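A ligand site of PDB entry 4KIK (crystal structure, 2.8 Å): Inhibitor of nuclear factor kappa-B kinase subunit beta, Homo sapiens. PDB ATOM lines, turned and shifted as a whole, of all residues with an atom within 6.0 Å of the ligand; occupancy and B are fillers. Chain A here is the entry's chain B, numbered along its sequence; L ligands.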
ATOM      1  N   LEU A  27       6.894  -9.578   4.683  1.00  0.00           N
ATOM      2  CA  LEU A  27       7.773  -9.132   3.620  1.00  0.00           C
ATOM      3  C   LEU A  27       8.255  -7.703   3.909  1.00  0.00           C
ATOM      4  O   LEU A  27       9.417  -7.390   3.621  1.00  0.00           O
ATOM      5  CB  LEU A  27       7.088  -9.285   2.262  1.00  0.00           C
ATOM      6  CG  LEU A  27       6.738 -10.749   1.875  1.00  0.00           C
ATOM      7  CD1 LEU A  27       5.942 -10.808   0.646  1.00  0.00           C
ATOM      8  CD2 LEU A  27       7.964 -11.605   1.674  1.00  0.00           C
ATOM      9  N   GLY A  28       7.424  -6.896   4.598  1.00  0.00           N
ATOM     10  CA  GLY A  28       7.784  -5.545   5.033  1.00  0.00           C
ATOM     11  C   GLY A  28       8.934  -5.508   6.039  1.00  0.00           C
ATOM     12  O   GLY A  28       9.491  -6.555   6.390  1.00  0.00           O
ATOM     13  N   THR A  29       9.281  -4.308   6.540  1.00  0.00           N
ATOM     14  CA  THR A  29      10.385  -4.159   7.508  1.00  0.00           C
ATOM     15  C   THR A  29       9.889  -3.677   8.897  1.00  0.00           C
ATOM     16  O   THR A  29      10.217  -4.304   9.902  1.00  0.00           O
ATOM     17  CB  THR A  29      11.533  -3.285   6.930  1.00  0.00           C
ATOM     18  OG1 THR A  29      12.432  -2.910   7.977  1.00  0.00           O
ATOM     19  CG2 THR A  29      11.039  -2.053   6.153  1.00  0.00           C
ATOM     20  N   ASN A  34       2.094  -5.604   7.239  1.00  0.00           N
ATOM     21  CA  ASN A  34       1.017  -5.441   6.268  1.00  0.00           C
ATOM     22  C   ASN A  34       1.113  -6.368   5.081  1.00  0.00           C
ATOM     23  O   ASN A  34       0.053  -6.800   4.609  1.00  0.00           O
ATOM     24  CB  ASN A  34       0.911  -4.013   5.764  1.00  0.00           C
ATOM     25  CG  ASN A  34       2.090  -3.497   5.020  1.00  0.00           C
ATOM     26  OD1 ASN A  34       3.242  -3.527   5.484  1.00  0.00           O
ATOM     27  ND2 ASN A  34       1.792  -2.909   3.884  1.00  0.00           N
ATOM     28  N   VAL A  35       2.339  -6.688   4.601  1.00  0.00           N
ATOM     29  CA  VAL A  35       2.555  -7.622   3.497  1.00  0.00           C
ATOM     30  C   VAL A  35       3.230  -8.902   4.046  1.00  0.00           C
ATOM     31  O   VAL A  35       4.298  -8.809   4.672  1.00  0.00           O
ATOM     32  CB  VAL A  35       3.330  -7.004   2.295  1.00  0.00           C
ATOM     33  CG1 VAL A  35       3.391  -7.989   1.117  1.00  0.00           C
ATOM     34  CG2 VAL A  35       2.695  -5.699   1.858  1.00  0.00           C
ATOM     35  N   ALA A  48       2.050 -13.035  -2.195  1.00  0.00           N
ATOM     36  CA  ALA A  48       2.235 -11.941  -1.218  1.00  0.00           C
ATOM     37  C   ALA A  48       0.840 -11.348  -0.887  1.00  0.00           C
ATOM     38  O   ALA A  48       0.081 -11.053  -1.828  1.00  0.00           O
ATOM     39  CB  ALA A  48       3.175 -10.891  -1.787  1.00  0.00           C
ATOM     40  N   LYS A  50      -1.292  -8.246   0.790  1.00  0.00           N
ATOM     41  CA  LYS A  50      -1.349  -6.959   1.444  1.00  0.00           C
ATOM     42  C   LYS A  50      -2.723  -6.865   2.117  1.00  0.00           C
ATOM     43  O   LYS A  50      -3.749  -7.156   1.498  1.00  0.00           O
ATOM     44  CB  LYS A  50      -1.085  -5.791   0.483  1.00  0.00           C
ATOM     45  CG  LYS A  50      -0.813  -4.487   1.245  1.00  0.00           C
ATOM     46  CD  LYS A  50      -0.199  -3.393   0.420  1.00  0.00           C
ATOM     47  CE  LYS A  50      -0.892  -2.093   0.721  1.00  0.00           C
ATOM     48  NZ  LYS A  50      -0.273  -0.939   0.027  1.00  0.00           N
ATOM     49  N   GLU A  67      -6.970   1.814  -4.145  1.00  0.00           N
ATOM     50  CA  GLU A  67      -5.787   0.991  -4.426  1.00  0.00           C
ATOM     51  C   GLU A  67      -6.184  -0.347  -5.062  1.00  0.00           C
ATOM     52  O   GLU A  67      -5.605  -0.719  -6.077  1.00  0.00           O
ATOM     53  CB  GLU A  67      -4.993   0.753  -3.143  1.00  0.00           C
ATOM     54  CG  GLU A  67      -3.687  -0.004  -3.380  1.00  0.00           C
ATOM     55  CD  GLU A  67      -2.891  -0.502  -2.192  1.00  0.00           C
ATOM     56  OE1 GLU A  67      -3.040   0.084  -1.093  1.00  0.00           O
ATOM     57  OE2 GLU A  67      -2.027  -1.385  -2.391  1.00  0.00           O
ATOM     58  N   VAL A  80       3.717  -5.494 -10.622  1.00  0.00           N
ATOM     59  CA  VAL A  80       3.193  -6.684  -9.936  1.00  0.00           C
ATOM     60  C   VAL A  80       1.666  -6.646 -10.009  1.00  0.00           C
ATOM     61  O   VAL A  80       1.009  -5.691  -9.554  1.00  0.00           O
ATOM     62  CB  VAL A  80       3.729  -6.862  -8.498  1.00  0.00           C
ATOM     63  CG1 VAL A  80       2.956  -7.926  -7.725  1.00  0.00           C
ATOM     64  CG2 VAL A  80       5.201  -7.219  -8.523  1.00  0.00           C
ATOM     65  N   LEU A 100      -5.270  -7.882  -0.810  1.00  0.00           N
ATOM     66  CA  LEU A 100      -4.596  -7.719  -2.083  1.00  0.00           C
ATOM     67  C   LEU A 100      -3.634  -8.872  -2.245  1.00  0.00           C
ATOM     68  O   LEU A 100      -2.550  -8.875  -1.651  1.00  0.00           O
ATOM     69  CB  LEU A 100      -3.888  -6.345  -2.190  1.00  0.00           C
ATOM     70  CG  LEU A 100      -3.143  -6.030  -3.488  1.00  0.00           C
ATOM     71  CD1 LEU A 100      -4.050  -6.195  -4.722  1.00  0.00           C
ATOM     72  CD2 LEU A 100      -2.491  -4.634  -3.416  1.00  0.00           C
ATOM     73  N   MET A 102      -1.011 -10.854  -4.399  1.00  0.00           N
ATOM     74  CA  MET A 102      -0.057 -10.526  -5.462  1.00  0.00           C
ATOM     75  C   MET A 102       0.940 -11.657  -5.673  1.00  0.00           C
ATOM     76  O   MET A 102       1.129 -12.490  -4.775  1.00  0.00           O
ATOM     77  CB  MET A 102       0.723  -9.252  -5.129  1.00  0.00           C
ATOM     78  CG  MET A 102      -0.111  -8.017  -5.023  1.00  0.00           C
ATOM     79  SD  MET A 102       0.708  -6.805  -4.010  1.00  0.00           S
ATOM     80  CE  MET A 102       0.615  -7.608  -2.358  1.00  0.00           C
ATOM     81  N   GLU A 103       1.619 -11.657  -6.819  1.00  0.00           N
ATOM     82  CA  GLU A 103       2.678 -12.618  -7.115  1.00  0.00           C
ATOM     83  C   GLU A 103       3.872 -12.387  -6.154  1.00  0.00           C
ATOM     84  O   GLU A 103       4.143 -11.247  -5.775  1.00  0.00           O
ATOM     85  CB  GLU A 103       3.122 -12.528  -8.614  1.00  0.00           C
ATOM     86  CG  GLU A 103       4.255 -11.570  -8.940  1.00  0.00           C
ATOM     87  CD  GLU A 103       4.412 -11.178 -10.400  1.00  0.00           C
ATOM     88  OE1 GLU A 103       3.923 -10.088 -10.759  1.00  0.00           O
ATOM     89  OE2 GLU A 103       5.035 -11.950 -11.172  1.00  0.00           O
ATOM     90  N   TYR A 104       4.558 -13.471  -5.770  1.00  0.00           N
ATOM     91  CA  TYR A 104       5.753 -13.345  -4.942  1.00  0.00           C
ATOM     92  C   TYR A 104       6.973 -13.276  -5.854  1.00  0.00           C
ATOM     93  O   TYR A 104       7.145 -14.097  -6.747  1.00  0.00           O
ATOM     94  CB  TYR A 104       5.880 -14.479  -3.911  1.00  0.00           C
ATOM     95  CG  TYR A 104       7.180 -14.441  -3.142  1.00  0.00           C
ATOM     96  CD1 TYR A 104       8.128 -15.460  -3.302  1.00  0.00           C
ATOM     97  CD2 TYR A 104       7.488 -13.386  -2.294  1.00  0.00           C
ATOM     98  CE1 TYR A 104       9.349 -15.424  -2.624  1.00  0.00           C
ATOM     99  CE2 TYR A 104       8.713 -13.335  -1.626  1.00  0.00           C
ATOM    100  CZ  TYR A 104       9.639 -14.357  -1.786  1.00  0.00           C
ATOM    101  OH  TYR A 104      10.828 -14.306  -1.139  1.00  0.00           O
ATOM    102  N   CYS A 105       7.799 -12.256  -5.656  1.00  0.00           N
ATOM    103  CA  CYS A 105       9.004 -11.983  -6.444  1.00  0.00           C
ATOM    104  C   CYS A 105      10.235 -12.416  -5.646  1.00  0.00           C
ATOM    105  O   CYS A 105      10.680 -11.748  -4.713  1.00  0.00           O
ATOM    106  CB  CYS A 105       9.052 -10.506  -6.834  1.00  0.00           C
ATOM    107  SG  CYS A 105       7.595  -9.933  -7.755  1.00  0.00           S
ATOM    108  N   GLN A 106      10.737 -13.599  -6.009  1.00  0.00           N
ATOM    109  CA  GLN A 106      11.868 -14.330  -5.429  1.00  0.00           C
ATOM    110  C   GLN A 106      13.224 -13.576  -5.364  1.00  0.00           C
ATOM    111  O   GLN A 106      14.030 -13.887  -4.482  1.00  0.00           O
ATOM    112  CB  GLN A 106      12.082 -15.634  -6.200  1.00  0.00           C
ATOM    113  CG  GLN A 106      11.086 -16.719  -5.813  1.00  0.00           C
ATOM    114  CD  GLN A 106      10.941 -17.739  -6.897  1.00  0.00           C
ATOM    115  OE1 GLN A 106       9.976 -17.707  -7.668  1.00  0.00           O
ATOM    116  NE2 GLN A 106      11.888 -18.666  -6.985  1.00  0.00           N
ATOM    117  N   GLY A 107      13.479 -12.639  -6.300  1.00  0.00           N
ATOM    118  CA  GLY A 107      14.702 -11.839  -6.318  1.00  0.00           C
ATOM    119  C   GLY A 107      14.801 -10.883  -5.136  1.00  0.00           C
ATOM    120  O   GLY A 107      15.908 -10.503  -4.724  1.00  0.00           O
ATOM    121  N   GLY A 108      13.656 -10.548  -4.564  1.00  0.00           N
ATOM    122  CA  GLY A 108      13.564  -9.642  -3.437  1.00  0.00           C
ATOM    123  C   GLY A 108      13.549  -8.192  -3.889  1.00  0.00           C
ATOM    124  O   GLY A 108      13.575  -7.907  -5.093  1.00  0.00           O
ATOM    125  N   ASP A 109      13.536  -7.271  -2.930  1.00  0.00           N
ATOM    126  CA  ASP A 109      13.488  -5.854  -3.233  1.00  0.00           C
ATOM    127  C   ASP A 109      14.879  -5.277  -3.672  1.00  0.00           C
ATOM    128  O   ASP A 109      15.926  -5.893  -3.441  1.00  0.00           O
ATOM    129  CB  ASP A 109      12.909  -5.080  -2.020  1.00  0.00           C
ATOM    130  CG  ASP A 109      13.728  -5.208  -0.754  1.00  0.00           C
ATOM    131  OD1 ASP A 109      14.084  -4.157  -0.185  1.00  0.00           O
ATOM    132  OD2 ASP A 109      14.020  -6.364  -0.331  1.00  0.00           O
ATOM    133  N   LYS A 153      10.580   4.237  -4.876  1.00  0.00           N
ATOM    134  CA  LYS A 153      11.851   4.080  -4.161  1.00  0.00           C
ATOM    135  C   LYS A 153      12.372   2.611  -4.269  1.00  0.00           C
ATOM    136  O   LYS A 153      11.584   1.746  -4.654  1.00  0.00           O
ATOM    137  CB  LYS A 153      11.679   4.495  -2.666  1.00  0.00           C
ATOM    138  CG  LYS A 153      10.757   3.608  -1.863  1.00  0.00           C
ATOM    139  CD  LYS A 153      10.258   4.291  -0.640  1.00  0.00           C
ATOM    140  CE  LYS A 153       9.276   3.391   0.061  1.00  0.00           C
ATOM    141  NZ  LYS A 153       8.796   3.967   1.343  1.00  0.00           N
ATOM    142  N   GLU A 155      12.629   0.262  -2.159  1.00  0.00           N
ATOM    143  CA  GLU A 155      11.757  -0.593  -1.345  1.00  0.00           C
ATOM    144  C   GLU A 155      10.474  -0.940  -2.090  1.00  0.00           C
ATOM    145  O   GLU A 155       9.784  -1.889  -1.724  1.00  0.00           O
ATOM    146  CB  GLU A 155      11.398   0.107  -0.028  1.00  0.00           C
ATOM    147  CG  GLU A 155      12.582   0.225   0.930  1.00  0.00           C
ATOM    148  CD  GLU A 155      13.492   1.431   0.804  1.00  0.00           C
ATOM    149  OE1 GLU A 155      13.411   2.155  -0.224  1.00  0.00           O
ATOM    150  OE2 GLU A 155      14.289   1.635   1.736  1.00  0.00           O
ATOM    151  N   ASN A 156      10.146  -0.159  -3.142  1.00  0.00           N
ATOM    152  CA  ASN A 156       8.941  -0.326  -3.942  1.00  0.00           C
ATOM    153  C   ASN A 156       9.236  -0.924  -5.308  1.00  0.00           C
ATOM    154  O   ASN A 156       8.384  -0.914  -6.197  1.00  0.00           O
ATOM    155  CB  ASN A 156       8.179   0.992  -4.052  1.00  0.00           C
ATOM    156  CG  ASN A 156       7.360   1.245  -2.815  1.00  0.00           C
ATOM    157  OD1 ASN A 156       7.341   0.458  -1.850  1.00  0.00           O
ATOM    158  ND2 ASN A 156       6.616   2.325  -2.829  1.00  0.00           N
ATOM    159  N   ILE A 157      10.444  -1.495  -5.443  1.00  0.00           N
ATOM    160  CA  ILE A 157      10.914  -2.208  -6.628  1.00  0.00           C
ATOM    161  C   ILE A 157      11.341  -3.598  -6.166  1.00  0.00           C
ATOM    162  O   ILE A 157      12.154  -3.715  -5.250  1.00  0.00           O
ATOM    163  CB  ILE A 157      12.054  -1.444  -7.368  1.00  0.00           C
ATOM    164  CG1 ILE A 157      11.528  -0.081  -7.933  1.00  0.00           C
ATOM    165  CG2 ILE A 157      12.728  -2.336  -8.452  1.00  0.00           C
ATOM    166  CD1 ILE A 157      12.555   0.835  -8.522  1.00  0.00           C
ATOM    167  N   VAL A 158      10.736  -4.630  -6.750  1.00  0.00           N
ATOM    168  CA  VAL A 158      11.050  -6.020  -6.421  1.00  0.00           C
ATOM    169  C   VAL A 158      11.527  -6.704  -7.695  1.00  0.00           C
ATOM    170  O   VAL A 158      11.186  -6.274  -8.804  1.00  0.00           O
ATOM    171  CB  VAL A 158       9.923  -6.822  -5.701  1.00  0.00           C
ATOM    172  CG1 VAL A 158       9.799  -6.389  -4.245  1.00  0.00           C
ATOM    173  CG2 VAL A 158       8.589  -6.716  -6.428  1.00  0.00           C
ATOM    174  N   ILE A 171       5.786  -2.142  -7.198  1.00  0.00           N
ATOM    175  CA  ILE A 171       4.828  -2.555  -6.187  1.00  0.00           C
ATOM    176  C   ILE A 171       4.309  -1.290  -5.473  1.00  0.00           C
ATOM    177  O   ILE A 171       4.724  -0.172  -5.791  1.00  0.00           O
ATOM    178  CB  ILE A 171       5.418  -3.632  -5.205  1.00  0.00           C
ATOM    179  CG1 ILE A 171       6.869  -3.365  -4.798  1.00  0.00           C
ATOM    180  CG2 ILE A 171       5.305  -4.990  -5.815  1.00  0.00           C
ATOM    181  CD1 ILE A 171       7.244  -3.751  -3.387  1.00  0.00           C
ATOM    182  N   ASP A 172       3.377  -1.496  -4.527  1.00  0.00           N
ATOM    183  CA  ASP A 172       2.783  -0.517  -3.609  1.00  0.00           C
ATOM    184  C   ASP A 172       2.123   0.656  -4.321  1.00  0.00           C
ATOM    185  O   ASP A 172       2.745   1.703  -4.536  1.00  0.00           O
ATOM    186  CB  ASP A 172       3.790  -0.015  -2.547  1.00  0.00           C
ATOM    187  CG  ASP A 172       3.130   0.625  -1.338  1.00  0.00           C
ATOM    188  OD1 ASP A 172       2.140   0.065  -0.831  1.00  0.00           O
ATOM    189  OD2 ASP A 172       3.581   1.702  -0.907  1.00  0.00           O
ATOM    190  N   LEU A 173       0.841   0.507  -4.612  1.00  0.00           N
ATOM    191  CA  LEU A 173       0.074   1.564  -5.248  1.00  0.00           C
ATOM    192  C   LEU A 173      -0.858   2.210  -4.194  1.00  0.00           C
ATOM    193  O   LEU A 173      -1.941   2.721  -4.508  1.00  0.00           O
ATOM    194  CB  LEU A 173      -0.688   0.982  -6.476  1.00  0.00           C
ATOM    195  CG  LEU A 173       0.072   0.774  -7.824  1.00  0.00           C
ATOM    196  CD1 LEU A 173       0.690   2.069  -8.365  1.00  0.00           C
ATOM    197  CD2 LEU A 173       1.068  -0.371  -7.776  1.00  0.00           C
HETATM  198  O1  LIG L   1       9.450  -3.361   2.781  1.00  0.00           O
HETATM  199  C1  LIG L   1       8.859  -2.830   1.879  1.00  0.00           C
HETATM  200  O2  LIG L   1       8.630  -1.530   1.800  1.00  0.00           O
HETATM  201  C2  LIG L   1       9.128  -0.712   2.887  1.00  0.00           C
HETATM  202  C3  LIG L   1       8.268  -3.588   0.670  1.00  0.00           C
HETATM  203  O3  LIG L   1       7.785  -2.716  -0.343  1.00  0.00           O
HETATM  204  C4  LIG L   1       7.048  -4.543   1.045  1.00  0.00           C
HETATM  205  O4  LIG L   1       7.806  -5.616   1.560  1.00  0.00           O
HETATM  206  C5  LIG L   1       6.149  -4.102   2.195  1.00  0.00           C
HETATM  207  N1  LIG L   1       6.191  -5.031  -0.164  1.00  0.00           N
HETATM  208  C6  LIG L   1       6.443  -6.229  -0.893  1.00  0.00           C
HETATM  209  C7  LIG L   1       7.556  -7.110  -0.826  1.00  0.00           C
HETATM  210  N2  LIG L   1       8.720  -7.004  -0.088  1.00  0.00           N
HETATM  211  C8  LIG L   1       9.009  -5.867   0.831  1.00  0.00           C
HETATM  212  C9  LIG L   1       9.343  -4.561   0.124  1.00  0.00           C
HETATM  213  C10 LIG L   1       9.548  -8.087  -0.422  1.00  0.00           C
HETATM  214  C11 LIG L   1      10.774  -8.461   0.107  1.00  0.00           C
HETATM  215  C12 LIG L   1      11.388  -9.608  -0.373  1.00  0.00           C
HETATM  216  C13 LIG L   1      10.796 -10.357  -1.381  1.00  0.00           C
HETATM  217  C14 LIG L   1       9.570  -9.983  -1.910  1.00  0.00           C
HETATM  218  C15 LIG L   1       8.917  -8.849  -1.422  1.00  0.00           C
HETATM  219  C16 LIG L   1       7.632  -8.229  -1.677  1.00  0.00           C
HETATM  220  C17 LIG L   1       6.581  -8.429  -2.584  1.00  0.00           C
HETATM  221  C18 LIG L   1       6.329  -9.530  -3.532  1.00  0.00           C
HETATM  222  O5  LIG L   1       7.007 -10.531  -3.748  1.00  0.00           O
HETATM  223  C19 LIG L   1       5.502  -7.561  -2.691  1.00  0.00           C
HETATM  224  C20 LIG L   1       4.548  -8.018  -3.761  1.00  0.00           C
HETATM  225  N3  LIG L   1       5.159  -9.274  -4.203  1.00  0.00           N
HETATM  226  C21 LIG L   1       5.435  -6.437  -1.849  1.00  0.00           C
HETATM  227  C22 LIG L   1       4.518  -5.314  -1.747  1.00  0.00           C
HETATM  228  C23 LIG L   1       5.001  -4.469  -0.729  1.00  0.00           C
HETATM  229  C24 LIG L   1       4.330  -3.298  -0.400  1.00  0.00           C
HETATM  230  C25 LIG L   1       3.347  -4.963  -2.415  1.00  0.00           C
HETATM  231  C26 LIG L   1       2.658  -3.803  -2.067  1.00  0.00           C
HETATM  232  C27 LIG L   1       3.144  -2.980  -1.060  1.00  0.00           C
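O of Glu 155 is in hydrogen-bond range of O3 of the ligand, 2.6 Å away.
N of Cys 105 sits at hydrogen-bond distance from O5 of the ligand (2.7 Å).
A nitrogen (N3) of the ligand is in hydrogen-bond range of the backbone carbonyl oxygen of Glu 103, 2.7 Å away.
N of Gly 28 sits at hydrogen-bond distance from O4 of the ligand (3.3 Å).
The backbone carbonyl oxygen of Val 35 lies within hydrogen-bond range of the backbone NH of Leu 27, 2.7 Å away.
NZ of Lys 50 is in salt-bridge range of OD1 of Asp 172 (2.8 Å).
The backbone carbonyl oxygen of Asn 156 is in hydrogen-bond range of the backbone NH of Ile 171 (3.0 Å).
The backbone NH (N) of Ala 48 sits at hydrogen-bond distance from the backbone carbonyl oxygen (O) of Met 102 (2.8 Å).
The side-chain amino group (NZ) of Lys 50 is in salt-bridge range of the side-chain carboxylate (OE2) of Glu 67 (3.0 Å).
The backbone carbonyl oxygen (O) of Leu 100 sits at hydrogen-bond distance from the backbone NH (N) of Lys 50 (2.8 Å).
An oxygen (O4) of the ligand lies close to the backbone carbonyl oxygen of Leu 27.
Residues that only touch the ligand: Asp 172 (3.2 Å), Tyr 104 (3.2 Å), Ile 171 (3.3 Å), Ala 48 (3.5 Å), Gly 108 (3.5 Å), Asn 156 (3.5 Å), Met 102 (3.6 Å), Val 35 (3.7 Å), Lys 50 (3.7 Å), Val 158 (3.8 Å), Thr 29 (3.9 Å) and Asp 109 (3.9 Å).
Hydrophobic or aromatic side chains that line the ligand: Leu 27, Val 35, Ala 48, Met 102, Tyr 104, Val 158 and Ile 171.
Of the 26 residues printed, 17 come within 4 Å of the ligand.
The nearest printed residue that does not touch the ligand is Val 80 (4.3 Å).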
